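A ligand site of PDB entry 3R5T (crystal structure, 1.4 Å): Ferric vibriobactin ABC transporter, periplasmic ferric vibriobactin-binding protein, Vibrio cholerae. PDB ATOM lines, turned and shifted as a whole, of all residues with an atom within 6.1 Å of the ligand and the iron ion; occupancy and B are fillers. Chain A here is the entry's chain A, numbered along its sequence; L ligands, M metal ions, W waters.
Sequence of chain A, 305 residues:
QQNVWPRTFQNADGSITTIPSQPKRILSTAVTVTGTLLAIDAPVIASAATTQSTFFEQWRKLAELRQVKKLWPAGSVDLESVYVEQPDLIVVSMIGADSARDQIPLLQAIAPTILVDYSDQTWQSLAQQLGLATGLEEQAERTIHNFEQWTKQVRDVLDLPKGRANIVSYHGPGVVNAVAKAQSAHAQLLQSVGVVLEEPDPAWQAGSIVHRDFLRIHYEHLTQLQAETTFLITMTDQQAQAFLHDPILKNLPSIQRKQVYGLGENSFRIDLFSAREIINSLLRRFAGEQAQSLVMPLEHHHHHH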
ATOM      1  N   VAL A  31     -23.273 -19.074  16.009  1.00  0.00           N
ATOM      2  CA  VAL A  31     -24.037 -17.849  16.191  1.00  0.00           C
ATOM      3  C   VAL A  31     -23.393 -16.653  15.453  1.00  0.00           C
ATOM      4  O   VAL A  31     -24.098 -15.795  14.915  1.00  0.00           O
ATOM      5  CB  VAL A  31     -24.253 -17.569  17.709  1.00  0.00           C
ATOM      6  CG1 VAL A  31     -22.914 -17.270  18.406  1.00  0.00           C
ATOM      7  CG2 VAL A  31     -25.271 -16.444  17.945  1.00  0.00           C
ATOM      8  N   THR A  32     -22.064 -16.605  15.395  1.00  0.00           N
ATOM      9  CA  THR A  32     -21.409 -15.522  14.651  1.00  0.00           C
ATOM     10  C   THR A  32     -21.827 -15.496  13.188  1.00  0.00           C
ATOM     11  O   THR A  32     -22.064 -14.438  12.638  1.00  0.00           O
ATOM     12  CB  THR A  32     -19.868 -15.607  14.698  1.00  0.00           C
ATOM     13  OG1 THR A  32     -19.441 -15.533  16.056  1.00  0.00           O
ATOM     14  CG2 THR A  32     -19.226 -14.459  13.930  1.00  0.00           C
ATOM     15  N   THR A  50     -25.028 -18.254  21.582  1.00  0.00           N
ATOM     16  CA  THR A  50     -23.832 -18.065  22.423  1.00  0.00           C
ATOM     17  C   THR A  50     -23.785 -19.114  23.551  1.00  0.00           C
ATOM     18  O   THR A  50     -24.727 -19.864  23.719  1.00  0.00           O
ATOM     19  CB  THR A  50     -23.848 -16.682  23.081  1.00  0.00           C
ATOM     20  OG1 THR A  50     -24.978 -16.620  23.961  1.00  0.00           O
ATOM     21  CG2 THR A  50     -23.946 -15.592  22.023  1.00  0.00           C
ATOM     22  N   THR A  51     -22.691 -19.151  24.317  1.00  0.00           N
ATOM     23  CA  THR A  51     -22.597 -20.084  25.446  1.00  0.00           C
ATOM     24  C   THR A  51     -23.695 -19.788  26.470  1.00  0.00           C
ATOM     25  O   THR A  51     -24.118 -20.675  27.237  1.00  0.00           O
ATOM     26  CB  THR A  51     -21.219 -20.044  26.141  1.00  0.00           C
ATOM     27  OG1 THR A  51     -21.011 -18.744  26.707  1.00  0.00           O
ATOM     28  CG2 THR A  51     -20.107 -20.341  25.157  1.00  0.00           C
ATOM     29  N   GLN A  52     -24.156 -18.534  26.484  1.00  0.00           N
ATOM     30  CA  GLN A  52     -25.223 -18.079  27.374  1.00  0.00           C
ATOM     31  C   GLN A  52     -26.649 -18.229  26.790  1.00  0.00           C
ATOM     32  O   GLN A  52     -27.610 -17.661  27.296  1.00  0.00           O
ATOM     33  CB  GLN A  52     -24.991 -16.619  27.778  1.00  0.00           C
ATOM     34  CG  GLN A  52     -23.630 -16.360  28.445  1.00  0.00           C
ATOM     35  CD  GLN A  52     -22.513 -16.113  27.448  1.00  0.00           C
ATOM     36  OE1 GLN A  52     -22.754 -15.766  26.274  1.00  0.00           O
ATOM     37  NE2 GLN A  52     -21.264 -16.278  27.890  1.00  0.00           N
ATOM     38  N   THR A  54     -27.994 -17.122  23.958  1.00  0.00           N
ATOM     39  CA  THR A  54     -28.597 -15.950  23.355  1.00  0.00           C
ATOM     40  C   THR A  54     -28.220 -15.816  21.888  1.00  0.00           C
ATOM     41  O   THR A  54     -27.194 -16.346  21.451  1.00  0.00           O
ATOM     42  CB  THR A  54     -28.174 -14.658  24.080  1.00  0.00           C
ATOM     43  OG1 THR A  54     -26.751 -14.504  24.007  1.00  0.00           O
ATOM     44  CG2 THR A  54     -28.618 -14.704  25.556  1.00  0.00           C
ATOM     45  N   PHE A  56     -27.273 -12.796  19.090  1.00  0.00           N
ATOM     46  CA  PHE A  56     -26.715 -11.435  19.181  1.00  0.00           C
ATOM     47  C   PHE A  56     -27.806 -10.401  19.023  1.00  0.00           C
ATOM     48  O   PHE A  56     -28.654 -10.512  18.119  1.00  0.00           O
ATOM     49  CB  PHE A  56     -25.579 -11.192  18.163  1.00  0.00           C
ATOM     50  CG  PHE A  56     -24.325 -11.962  18.451  1.00  0.00           C
ATOM     51  CD1 PHE A  56     -23.771 -11.978  19.719  1.00  0.00           C
ATOM     52  CD2 PHE A  56     -23.693 -12.669  17.441  1.00  0.00           C
ATOM     53  CE1 PHE A  56     -22.594 -12.683  19.974  1.00  0.00           C
ATOM     54  CE2 PHE A  56     -22.511 -13.363  17.680  1.00  0.00           C
ATOM     55  CZ  PHE A  56     -21.980 -13.388  18.949  1.00  0.00           C
ATOM     56  N   ALA A  74     -23.576 -22.661  22.280  1.00  0.00           N
ATOM     57  CA  ALA A  74     -22.245 -23.074  21.840  1.00  0.00           C
ATOM     58  C   ALA A  74     -21.613 -24.091  22.780  1.00  0.00           C
ATOM     59  O   ALA A  74     -21.592 -23.900  24.000  1.00  0.00           O
ATOM     60  CB  ALA A  74     -21.349 -21.857  21.704  1.00  0.00           C
ATOM     61  N   ILE A  95     -12.991 -21.393  14.017  1.00  0.00           N
ATOM     62  CA  ILE A  95     -12.381 -21.043  15.311  1.00  0.00           C
ATOM     63  C   ILE A  95     -13.222 -20.022  16.061  1.00  0.00           C
ATOM     64  O   ILE A  95     -13.761 -19.085  15.453  1.00  0.00           O
ATOM     65  CB  ILE A  95     -10.933 -20.522  15.133  1.00  0.00           C
ATOM     66  CG1 ILE A  95     -10.298 -20.168  16.486  1.00  0.00           C
ATOM     67  CG2 ILE A  95     -10.919 -19.300  14.204  1.00  0.00           C
ATOM     68  CD1 ILE A  95      -8.772 -20.003  16.416  1.00  0.00           C
ATOM     69  N   GLY A  96     -13.317 -20.194  17.372  1.00  0.00           N
ATOM     70  CA  GLY A  96     -14.163 -19.340  18.188  1.00  0.00           C
ATOM     71  C   GLY A  96     -14.972 -20.212  19.137  1.00  0.00           C
ATOM     72  O   GLY A  96     -15.053 -21.431  18.940  1.00  0.00           O
ATOM     73  N   ALA A  97     -15.583 -19.608  20.137  1.00  0.00           N
ATOM     74  CA  ALA A  97     -16.380 -20.400  21.091  1.00  0.00           C
ATOM     75  C   ALA A  97     -17.533 -21.170  20.427  1.00  0.00           C
ATOM     76  O   ALA A  97     -18.006 -22.186  20.977  1.00  0.00           O
ATOM     77  CB  ALA A  97     -16.907 -19.512  22.232  1.00  0.00           C
ATOM     78  N   ASP A  98     -17.982 -20.674  19.282  1.00  0.00           N
ATOM     79  CA  ASP A  98     -19.116 -21.245  18.540  1.00  0.00           C
ATOM     80  C   ASP A  98     -18.700 -22.262  17.478  1.00  0.00           C
ATOM     81  O   ASP A  98     -19.528 -22.718  16.696  1.00  0.00           O
ATOM     82  CB  ASP A  98     -19.994 -20.126  17.916  1.00  0.00           C
ATOM     83  CG  ASP A  98     -19.233 -19.240  16.961  1.00  0.00           C
ATOM     84  OD1 ASP A  98     -18.071 -19.526  16.632  1.00  0.00           O
ATOM     85  OD2 ASP A  98     -19.827 -18.233  16.538  1.00  0.00           O
ATOM     86  N   SER A  99     -17.437 -22.664  17.487  1.00  0.00           N
ATOM     87  CA  SER A  99     -16.953 -23.648  16.515  1.00  0.00           C
ATOM     88  C   SER A  99     -17.391 -25.073  16.822  1.00  0.00           C
ATOM     89  O   SER A  99     -17.147 -25.576  17.924  1.00  0.00           O
ATOM     90  CB  SER A  99     -15.435 -23.601  16.393  1.00  0.00           C
ATOM     91  OG  SER A  99     -14.976 -24.624  15.511  1.00  0.00           O
ATOM     92  N   TYR A 118     -14.580 -16.956  10.084  1.00  0.00           N
ATOM     93  CA  TYR A 118     -14.985 -15.559  10.119  1.00  0.00           C
ATOM     94  C   TYR A 118     -13.932 -14.666  10.767  1.00  0.00           C
ATOM     95  O   TYR A 118     -14.096 -13.440  10.808  1.00  0.00           O
ATOM     96  CB  TYR A 118     -16.317 -15.387  10.823  1.00  0.00           C
ATOM     97  CG  TYR A 118     -16.342 -15.936  12.239  1.00  0.00           C
ATOM     98  CD1 TYR A 118     -15.576 -15.349  13.254  1.00  0.00           C
ATOM     99  CD2 TYR A 118     -17.146 -17.021  12.571  1.00  0.00           C
ATOM    100  CE1 TYR A 118     -15.599 -15.845  14.558  1.00  0.00           C
ATOM    101  CE2 TYR A 118     -17.175 -17.521  13.870  1.00  0.00           C
ATOM    102  CZ  TYR A 118     -16.415 -16.934  14.871  1.00  0.00           C
ATOM    103  OH  TYR A 118     -16.478 -17.435  16.159  1.00  0.00           O
ATOM    104  N   SER A 169     -10.538  -5.248  23.278  1.00  0.00           N
ATOM    105  CA  SER A 169     -11.459  -6.005  24.118  1.00  0.00           C
ATOM    106  C   SER A 169     -10.886  -5.996  25.529  1.00  0.00           C
ATOM    107  O   SER A 169      -9.870  -6.631  25.803  1.00  0.00           O
ATOM    108  CB  SER A 169     -11.617  -7.429  23.599  1.00  0.00           C
ATOM    109  OG  SER A 169     -12.545  -8.151  24.398  1.00  0.00           O
ATOM    110  N   TYR A 170     -11.526  -5.257  26.422  1.00  0.00           N
ATOM    111  CA  TYR A 170     -10.979  -4.977  27.751  1.00  0.00           C
ATOM    112  C   TYR A 170     -11.632  -5.781  28.850  1.00  0.00           C
ATOM    113  O   TYR A 170     -12.858  -5.840  28.933  1.00  0.00           O
ATOM    114  CB  TYR A 170     -11.129  -3.485  28.046  1.00  0.00           C
ATOM    115  CG  TYR A 170     -10.639  -3.029  29.404  1.00  0.00           C
ATOM    116  CD1 TYR A 170      -9.278  -2.950  29.680  1.00  0.00           C
ATOM    117  CD2 TYR A 170     -11.533  -2.612  30.384  1.00  0.00           C
ATOM    118  CE1 TYR A 170      -8.813  -2.489  30.912  1.00  0.00           C
ATOM    119  CE2 TYR A 170     -11.073  -2.162  31.633  1.00  0.00           C
ATOM    120  CZ  TYR A 170      -9.720  -2.111  31.888  1.00  0.00           C
ATOM    121  OH  TYR A 170      -9.282  -1.646  33.115  1.00  0.00           O
ATOM    122  N   HIS A 171     -10.799  -6.380  29.686  1.00  0.00           N
ATOM    123  CA  HIS A 171     -11.281  -7.142  30.841  1.00  0.00           C
ATOM    124  C   HIS A 171     -10.574  -6.785  32.132  1.00  0.00           C
ATOM    125  O   HIS A 171     -10.787  -7.442  33.131  1.00  0.00           O
ATOM    126  CB  HIS A 171     -11.171  -8.643  30.589  1.00  0.00           C
ATOM    127  CG  HIS A 171     -11.997  -9.102  29.440  1.00  0.00           C
ATOM    128  ND1 HIS A 171     -13.372  -9.195  29.505  1.00  0.00           N
ATOM    129  CD2 HIS A 171     -11.650  -9.458  28.183  1.00  0.00           C
ATOM    130  CE1 HIS A 171     -13.839  -9.594  28.334  1.00  0.00           C
ATOM    131  NE2 HIS A 171     -12.813  -9.758  27.516  1.00  0.00           N
ATOM    132  N   VAL A 176      -6.043 -11.787  30.724  1.00  0.00           N
ATOM    133  CA  VAL A 176      -5.636 -11.626  29.345  1.00  0.00           C
ATOM    134  C   VAL A 176      -6.653 -10.725  28.651  1.00  0.00           C
ATOM    135  O   VAL A 176      -7.854 -10.954  28.722  1.00  0.00           O
ATOM    136  CB  VAL A 176      -5.539 -12.997  28.622  1.00  0.00           C
ATOM    137  CG1 VAL A 176      -5.507 -12.811  27.093  1.00  0.00           C
ATOM    138  CG2 VAL A 176      -4.304 -13.755  29.118  1.00  0.00           C
ATOM    139  N   ASN A 177      -6.167  -9.663  28.001  1.00  0.00           N
ATOM    140  CA  ASN A 177      -7.016  -8.754  27.243  1.00  0.00           C
ATOM    141  C   ASN A 177      -6.761  -8.980  25.758  1.00  0.00           C
ATOM    142  O   ASN A 177      -5.964  -9.843  25.385  1.00  0.00           O
ATOM    143  CB  ASN A 177      -6.690  -7.294  27.617  1.00  0.00           C
ATOM    144  CG  ASN A 177      -7.238  -6.886  29.002  1.00  0.00           C
ATOM    145  OD1 ASN A 177      -8.097  -6.012  29.083  1.00  0.00           O
ATOM    146  ND2 ASN A 177      -6.748  -7.532  30.079  1.00  0.00           N
ATOM    147  N   ALA A 178      -7.373  -8.192  24.890  1.00  0.00           N
ATOM    148  CA  ALA A 178      -7.146  -8.435  23.459  1.00  0.00           C
ATOM    149  C   ALA A 178      -7.226  -7.176  22.621  1.00  0.00           C
ATOM    150  O   ALA A 178      -7.911  -6.221  22.989  1.00  0.00           O
ATOM    151  CB  ALA A 178      -8.106  -9.503  22.925  1.00  0.00           C
ATOM    152  N   ILE A 209      -2.070 -20.390  21.692  1.00  0.00           N
ATOM    153  CA  ILE A 209      -3.173 -20.395  20.727  1.00  0.00           C
ATOM    154  C   ILE A 209      -3.121 -19.199  19.770  1.00  0.00           C
ATOM    155  O   ILE A 209      -3.085 -18.044  20.205  1.00  0.00           O
ATOM    156  CB  ILE A 209      -4.536 -20.389  21.417  1.00  0.00           C
ATOM    157  CG1 ILE A 209      -4.640 -21.520  22.460  1.00  0.00           C
ATOM    158  CG2 ILE A 209      -5.653 -20.499  20.395  1.00  0.00           C
ATOM    159  CD1 ILE A 209      -4.516 -22.913  21.877  1.00  0.00           C
ATOM    160  N   HIS A 211      -4.623 -16.609  17.115  1.00  0.00           N
ATOM    161  CA  HIS A 211      -5.865 -15.969  16.701  1.00  0.00           C
ATOM    162  C   HIS A 211      -5.603 -14.932  15.625  1.00  0.00           C
ATOM    163  O   HIS A 211      -4.625 -14.177  15.714  1.00  0.00           O
ATOM    164  CB  HIS A 211      -6.533 -15.267  17.879  1.00  0.00           C
ATOM    165  CG  HIS A 211      -6.957 -16.182  18.982  1.00  0.00           C
ATOM    166  ND1 HIS A 211      -8.135 -16.899  18.939  1.00  0.00           N
ATOM    167  CD2 HIS A 211      -6.378 -16.470  20.162  1.00  0.00           C
ATOM    168  CE1 HIS A 211      -8.263 -17.589  20.065  1.00  0.00           C
ATOM    169  NE2 HIS A 211      -7.206 -17.344  20.812  1.00  0.00           N
ATOM    170  N   ASP A 213      -8.136 -12.715  14.549  1.00  0.00           N
ATOM    171  CA  ASP A 213      -9.039 -11.578  14.732  1.00  0.00           C
ATOM    172  C   ASP A 213      -8.529 -10.553  15.744  1.00  0.00           C
ATOM    173  O   ASP A 213      -8.289  -9.388  15.409  1.00  0.00           O
ATOM    174  CB  ASP A 213     -10.487 -12.052  15.060  1.00  0.00           C
ATOM    175  CG  ASP A 213     -10.601 -12.962  16.298  1.00  0.00           C
ATOM    176  OD1 ASP A 213      -9.616 -13.592  16.723  1.00  0.00           O
ATOM    177  OD2 ASP A 213     -11.731 -13.055  16.839  1.00  0.00           O
ATOM    178  N   PHE A 214      -8.380 -11.010  16.991  1.00  0.00           N
ATOM    179  CA  PHE A 214      -7.794 -10.179  18.040  1.00  0.00           C
ATOM    180  C   PHE A 214      -6.599 -10.904  18.618  1.00  0.00           C
ATOM    181  O   PHE A 214      -6.664 -12.108  18.885  1.00  0.00           O
ATOM    182  CB  PHE A 214      -8.808  -9.940  19.176  1.00  0.00           C
ATOM    183  CG  PHE A 214      -9.868  -8.912  18.865  1.00  0.00           C
ATOM    184  CD1 PHE A 214      -9.905  -7.711  19.550  1.00  0.00           C
ATOM    185  CD2 PHE A 214     -10.825  -9.154  17.884  1.00  0.00           C
ATOM    186  CE1 PHE A 214     -10.898  -6.770  19.267  1.00  0.00           C
ATOM    187  CE2 PHE A 214     -11.801  -8.210  17.596  1.00  0.00           C
ATOM    188  CZ  PHE A 214     -11.825  -7.011  18.283  1.00  0.00           C
ATOM    189  N   ARG A 216      -4.597 -11.914  21.604  1.00  0.00           N
ATOM    190  CA  ARG A 216      -4.752 -12.029  23.042  1.00  0.00           C
ATOM    191  C   ARG A 216      -3.406 -11.739  23.699  1.00  0.00           C
ATOM    192  O   ARG A 216      -2.378 -12.274  23.284  1.00  0.00           O
ATOM    193  CB  ARG A 216      -5.243 -13.437  23.404  1.00  0.00           C
ATOM    194  CG  ARG A 216      -6.750 -13.587  23.355  1.00  0.00           C
ATOM    195  CD  ARG A 216      -7.330 -13.364  21.988  1.00  0.00           C
ATOM    196  NE  ARG A 216      -8.648 -13.999  21.941  1.00  0.00           N
ATOM    197  CZ  ARG A 216      -9.392 -14.106  20.853  1.00  0.00           C
ATOM    198  NH1 ARG A 216      -8.993 -13.588  19.692  1.00  0.00           N
ATOM    199  NH2 ARG A 216     -10.578 -14.718  20.934  1.00  0.00           N
ATOM    200  N   ILE A 233     -14.645  -2.694  22.192  1.00  0.00           N
ATOM    201  CA  ILE A 233     -15.759  -3.527  21.744  1.00  0.00           C
ATOM    202  C   ILE A 233     -16.698  -3.881  22.889  1.00  0.00           C
ATOM    203  O   ILE A 233     -16.276  -3.915  24.045  1.00  0.00           O
ATOM    204  CB  ILE A 233     -15.294  -4.799  20.990  1.00  0.00           C
ATOM    205  CG1 ILE A 233     -14.581  -5.802  21.903  1.00  0.00           C
ATOM    206  CG2 ILE A 233     -14.450  -4.396  19.774  1.00  0.00           C
ATOM    207  CD1 ILE A 233     -14.426  -7.163  21.228  1.00  0.00           C
ATOM    208  N   PHE A 268     -19.621  -6.670  19.611  1.00  0.00           N
ATOM    209  CA  PHE A 268     -18.744  -7.809  19.869  1.00  0.00           C
ATOM    210  C   PHE A 268     -18.314  -8.522  18.562  1.00  0.00           C
ATOM    211  O   PHE A 268     -17.118  -8.688  18.306  1.00  0.00           O
ATOM    212  CB  PHE A 268     -19.337  -8.798  20.885  1.00  0.00           C
ATOM    213  CG  PHE A 268     -18.450  -9.968  21.140  1.00  0.00           C
ATOM    214  CD1 PHE A 268     -17.251  -9.792  21.814  1.00  0.00           C
ATOM    215  CD2 PHE A 268     -18.794 -11.217  20.672  1.00  0.00           C
ATOM    216  CE1 PHE A 268     -16.389 -10.848  22.035  1.00  0.00           C
ATOM    217  CE2 PHE A 268     -17.942 -12.295  20.888  1.00  0.00           C
ATOM    218  CZ  PHE A 268     -16.727 -12.104  21.565  1.00  0.00           C
ATOM    219  N   ARG A 269     -19.293  -8.912  17.750  1.00  0.00           N
ATOM    220  CA  ARG A 269     -19.005  -9.484  16.426  1.00  0.00           C
ATOM    221  C   ARG A 269     -19.552  -8.545  15.367  1.00  0.00           C
ATOM    222  O   ARG A 269     -20.538  -7.818  15.622  1.00  0.00           O
ATOM    223  CB  ARG A 269     -19.657 -10.860  16.284  1.00  0.00           C
ATOM    224  CG  ARG A 269     -18.971 -11.993  17.046  1.00  0.00           C
ATOM    225  CD  ARG A 269     -17.603 -12.323  16.499  1.00  0.00           C
ATOM    226  NE  ARG A 269     -17.164 -13.682  16.825  1.00  0.00           N
ATOM    227  CZ  ARG A 269     -16.294 -13.989  17.780  1.00  0.00           C
ATOM    228  NH1 ARG A 269     -15.738 -13.047  18.537  1.00  0.00           N
ATOM    229  NH2 ARG A 269     -15.945 -15.262  17.975  1.00  0.00           N
HETATM  230  C1  LIG L   1     -13.933 -15.777  25.810  1.00  0.00           C
HETATM  231  N1  LIG L   1     -14.440 -16.960  23.630  1.00  0.00           N
HETATM  232  O1  LIG L   1     -12.757 -15.801  25.623  1.00  0.00           O
HETATM  233  C2  LIG L   1     -14.890 -16.599  24.967  1.00  0.00           C
HETATM  234  C3  LIG L   1     -15.213 -18.015  25.571  1.00  0.00           C
HETATM  235  C4  LIG L   1     -21.534 -12.232  23.879  1.00  0.00           C
HETATM  236  O2  LIG L   1     -11.934 -10.692  24.958  1.00  0.00           O
HETATM  237  O3  LIG L   1     -19.126 -15.350  26.220  1.00  0.00           O
HETATM  238  O4  LIG L   1     -14.018 -14.166  20.504  1.00  0.00           O
HETATM  239  O5  LIG L   1     -11.378 -17.908  19.487  1.00  0.00           O
HETATM  240  O6  LIG L   1     -15.587 -16.760  20.527  1.00  0.00           O
HETATM  241  O7  LIG L   1     -13.707 -14.033  23.140  1.00  0.00           O
HETATM  242  O8  LIG L   1     -12.900 -16.798  21.445  1.00  0.00           O
HETATM  243  O9  LIG L   1     -16.551 -15.216  22.537  1.00  0.00           O
HETATM  244  C5  LIG L   1     -12.263 -10.865  20.782  1.00  0.00           C
HETATM  245  C6  LIG L   1     -12.010 -20.806  21.741  1.00  0.00           C
HETATM  246  C7  LIG L   1     -19.230 -16.788  19.796  1.00  0.00           C
HETATM  247  C8  LIG L   1     -12.901 -12.009  20.192  1.00  0.00           C
HETATM  248  C9  LIG L   1     -11.540 -20.057  20.635  1.00  0.00           C
HETATM  249  C10 LIG L   1     -17.827 -17.045  19.633  1.00  0.00           C
HETATM  250  C11 LIG L   1     -12.094 -10.790  22.219  1.00  0.00           C
HETATM  251  C12 LIG L   1     -12.770 -20.205  22.754  1.00  0.00           C
HETATM  252  C13 LIG L   1     -19.705 -16.035  20.895  1.00  0.00           C
HETATM  253  C14 LIG L   1     -13.085 -13.109  27.738  1.00  0.00           C
HETATM  254  C15 LIG L   1     -16.389 -14.100  28.315  1.00  0.00           C
HETATM  255  C16 LIG L   1     -11.978 -12.897  26.691  1.00  0.00           C
HETATM  256  C17 LIG L   1     -17.914 -13.920  28.406  1.00  0.00           C
HETATM  257  C18 LIG L   1     -13.531 -14.553  27.958  1.00  0.00           C
HETATM  258  C19 LIG L   1     -15.913 -15.105  27.256  1.00  0.00           C
HETATM  259  N2  LIG L   1     -12.381 -12.923  25.297  1.00  0.00           N
HETATM  260  N3  LIG L   1     -18.446 -13.319  27.178  1.00  0.00           N
HETATM  261  N4  LIG L   1     -18.461 -13.865  23.696  1.00  0.00           N
HETATM  262  O10 LIG L   1     -20.641 -14.454  23.082  1.00  0.00           O
HETATM  263  C20 LIG L   1     -12.295 -11.721  24.500  1.00  0.00           C
HETATM  264  C21 LIG L   1     -19.019 -14.164  26.124  1.00  0.00           C
HETATM  265  C22 LIG L   1     -13.708 -18.194  23.808  1.00  0.00           C
HETATM  266  C23 LIG L   1     -13.372 -13.061  21.024  1.00  0.00           C
HETATM  267  C24 LIG L   1     -11.828 -18.680  20.549  1.00  0.00           C
HETATM  268  C25 LIG L   1     -16.951 -16.532  20.587  1.00  0.00           C
HETATM  269  C26 LIG L   1     -13.203 -13.002  22.379  1.00  0.00           C
HETATM  270  C27 LIG L   1     -12.548 -18.111  21.518  1.00  0.00           C
HETATM  271  C28 LIG L   1     -17.423 -15.804  21.647  1.00  0.00           C
HETATM  272  C29 LIG L   1     -12.533 -11.809  22.997  1.00  0.00           C
HETATM  273  C30 LIG L   1     -13.059 -18.904  22.644  1.00  0.00           C
HETATM  274  C31 LIG L   1     -18.847 -15.521  21.795  1.00  0.00           C
HETATM  275  C32 LIG L   1     -20.811 -13.517  24.231  1.00  0.00           C
HETATM  276  C33 LIG L   1     -19.296 -14.819  23.041  1.00  0.00           C
HETATM  277  C34 LIG L   1     -19.309 -13.438  24.817  1.00  0.00           C
HETATM  278  N5  LIG L   1     -14.471 -15.091  26.981  1.00  0.00           N
HETATM  279  O11 LIG L   1     -14.251 -18.931  24.887  1.00  0.00           O
HETATM  280  C35 LIG L   1     -16.670 -18.444  25.657  1.00  0.00           C
HETATM  281 FE    FE M   1     -14.451 -15.628  21.958  1.00  0.00          FE
HETATM  282  O   HOH W   1     -12.176 -22.736  18.486  1.00  0.00           O
HETATM  283  O   HOH W   2     -20.210 -17.394  24.337  1.00  0.00           O
HETATM  284  O   HOH W   3     -15.038 -10.223  18.728  1.00  0.00           O
HETATM  285  O   HOH W   4     -24.229 -10.793  23.208  1.00  0.00           O
HETATM  286  O   HOH W   5      -9.114 -11.369  25.885  1.00  0.00           O
HETATM  287  O   HOH W   6     -15.847 -13.097  24.653  1.00  0.00           O
HETATM  288  O   HOH W   7      -9.873 -16.430  16.928  1.00  0.00           O
HETATM  289  O   HOH W   8      -9.612 -22.494  19.404  1.00  0.00           O
HETATM  290  O   HOH W   9     -18.263 -10.521  26.804  1.00  0.00           O
HETATM  291  O   HOH W  10     -12.315 -15.117  18.616  1.00  0.00           O
HETATM  292  O   HOH W  11     -21.699 -11.906  27.097  1.00  0.00           O
HETATM  293  O   HOH W  12     -22.037  -8.957  23.662  1.00  0.00           O
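O3 of the ligand is in hydrogen-bond range of NE2 of Gln 52, at 2.9 Å.
An oxygen (O2) of the ligand lies within hydrogen-bond range of a ring nitrogen (NE2) of His 171 (2.9 Å).
The guanidinium group (NH1) of Arg 269 lies close to an oxygen (O4) of the ligand (2.8 Å).
A ring nitrogen (ND1) of His 211 lies close to an oxygen (O5) of the ligand, 3.4 Å away.
The backbone NH (N) of Ala 97 lies close to an oxygen (O6) of the ligand, at 2.9 Å.
The guanidinium group (NH2) of Arg 216 sits close to an oxygen (O8) of the ligand (3.2 Å).
An oxygen (O2) of the ligand is in hydrogen-bond range of the side-chain hydroxyl (OG) of Ser 169, 2.7 Å away.
NH1 of Arg 216 lies within salt-bridge range of OD1 of Asp 213 (3.0 Å).
N of His 171 lies within hydrogen-bond range of OD1 of Asn 177 (2.8 Å).
The backbone carbonyl oxygen (O) of Phe 214 sits at hydrogen-bond distance from the guanidinium group (NH1) of Arg 216, at 2.9 Å.
N of Gln 52 lies close to OG1 of Thr 50 (3.3 Å).
The guanidinium group (NH2) of Arg 269 lies within hydrogen-bond range of the side-chain hydroxyl (OH) of Tyr 118, 2.9 Å away.
N of Ala 74 lies within hydrogen-bond range of O of Thr 50 (3.3 Å).
OD1 of Asp 98 is in hydrogen-bond range of OH of Tyr 118 (2.7 Å).
The side-chain hydroxyl (OH) of Tyr 118 lies within hydrogen-bond range of the backbone carbonyl oxygen (O) of Ile 95, 3.3 Å away.
Residues that only touch the ligand: Phe 268, Gly 96, Asp 98, Phe 214, Thr 50, Asp 213, Tyr 118, Ile 95, Thr 51, Thr 32, Val 31 and Phe 56.
Hydrophobic or aromatic side chains that line the ligand: Val 31, Phe 56, Ile 95, Ala 97, His 171, His 211, Phe 214 and Phe 268.
19 residues have an atom within 4 Å of the ligand: Val 31, Thr 32, Thr 50, Thr 51, Gln 52, Phe 56, Ile 95, Gly 96, Ala 97, Asp 98, Tyr 118, Ser 169, His 171, His 211, Asp 213, Phe 214, Arg 216, Phe 268 and Arg 269.
Along chain A the residues within 4 Å of the ligand span positions 31 to 269.
No residue comes within 4 Å of the iron ion.
The nearest printed residue that does not touch the iron ion is Arg 216 (4.1 Å).
The iron ion is bound by an oxygen (O8) of the ligand (2.0 Å), an oxygen (O4) of the ligand (2.1 Å), an oxygen (O7) of the ligand (2.1 Å), a nitrogen (N1) of the ligand (2.1 Å), an oxygen (O6) of the ligand (2.1 Å) and an oxygen (O9) of the ligand (2.2 Å).
The iron ion has six donor atoms within binding distance.
Water W10 lies within hydrogen-bond range of OD2 of Asp 213, NH2 of Arg 216 and O5 of the ligand.
Water W2 lies within hydrogen-bond range of OG1 of Thr 51 (2.8 Å) and O3 of the ligand (3.0 Å).
Water W5 bridges an oxygen (O2) of the ligand (3.0 Å) and the backbone carbonyl oxygen of Val 176 (3.1 Å).
Water W3 lies within hydrogen-bond range of the backbone carbonyl oxygen of Phe 268 (2.6 Å) and the guanidinium group of Arg 269 (2.9 Å).
Water W7 lies within hydrogen-bond range of ND1 of His 211 (2.7 Å), OD1 of Asp 213 (2.9 Å) and O5 of the ligand (3.3 Å).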
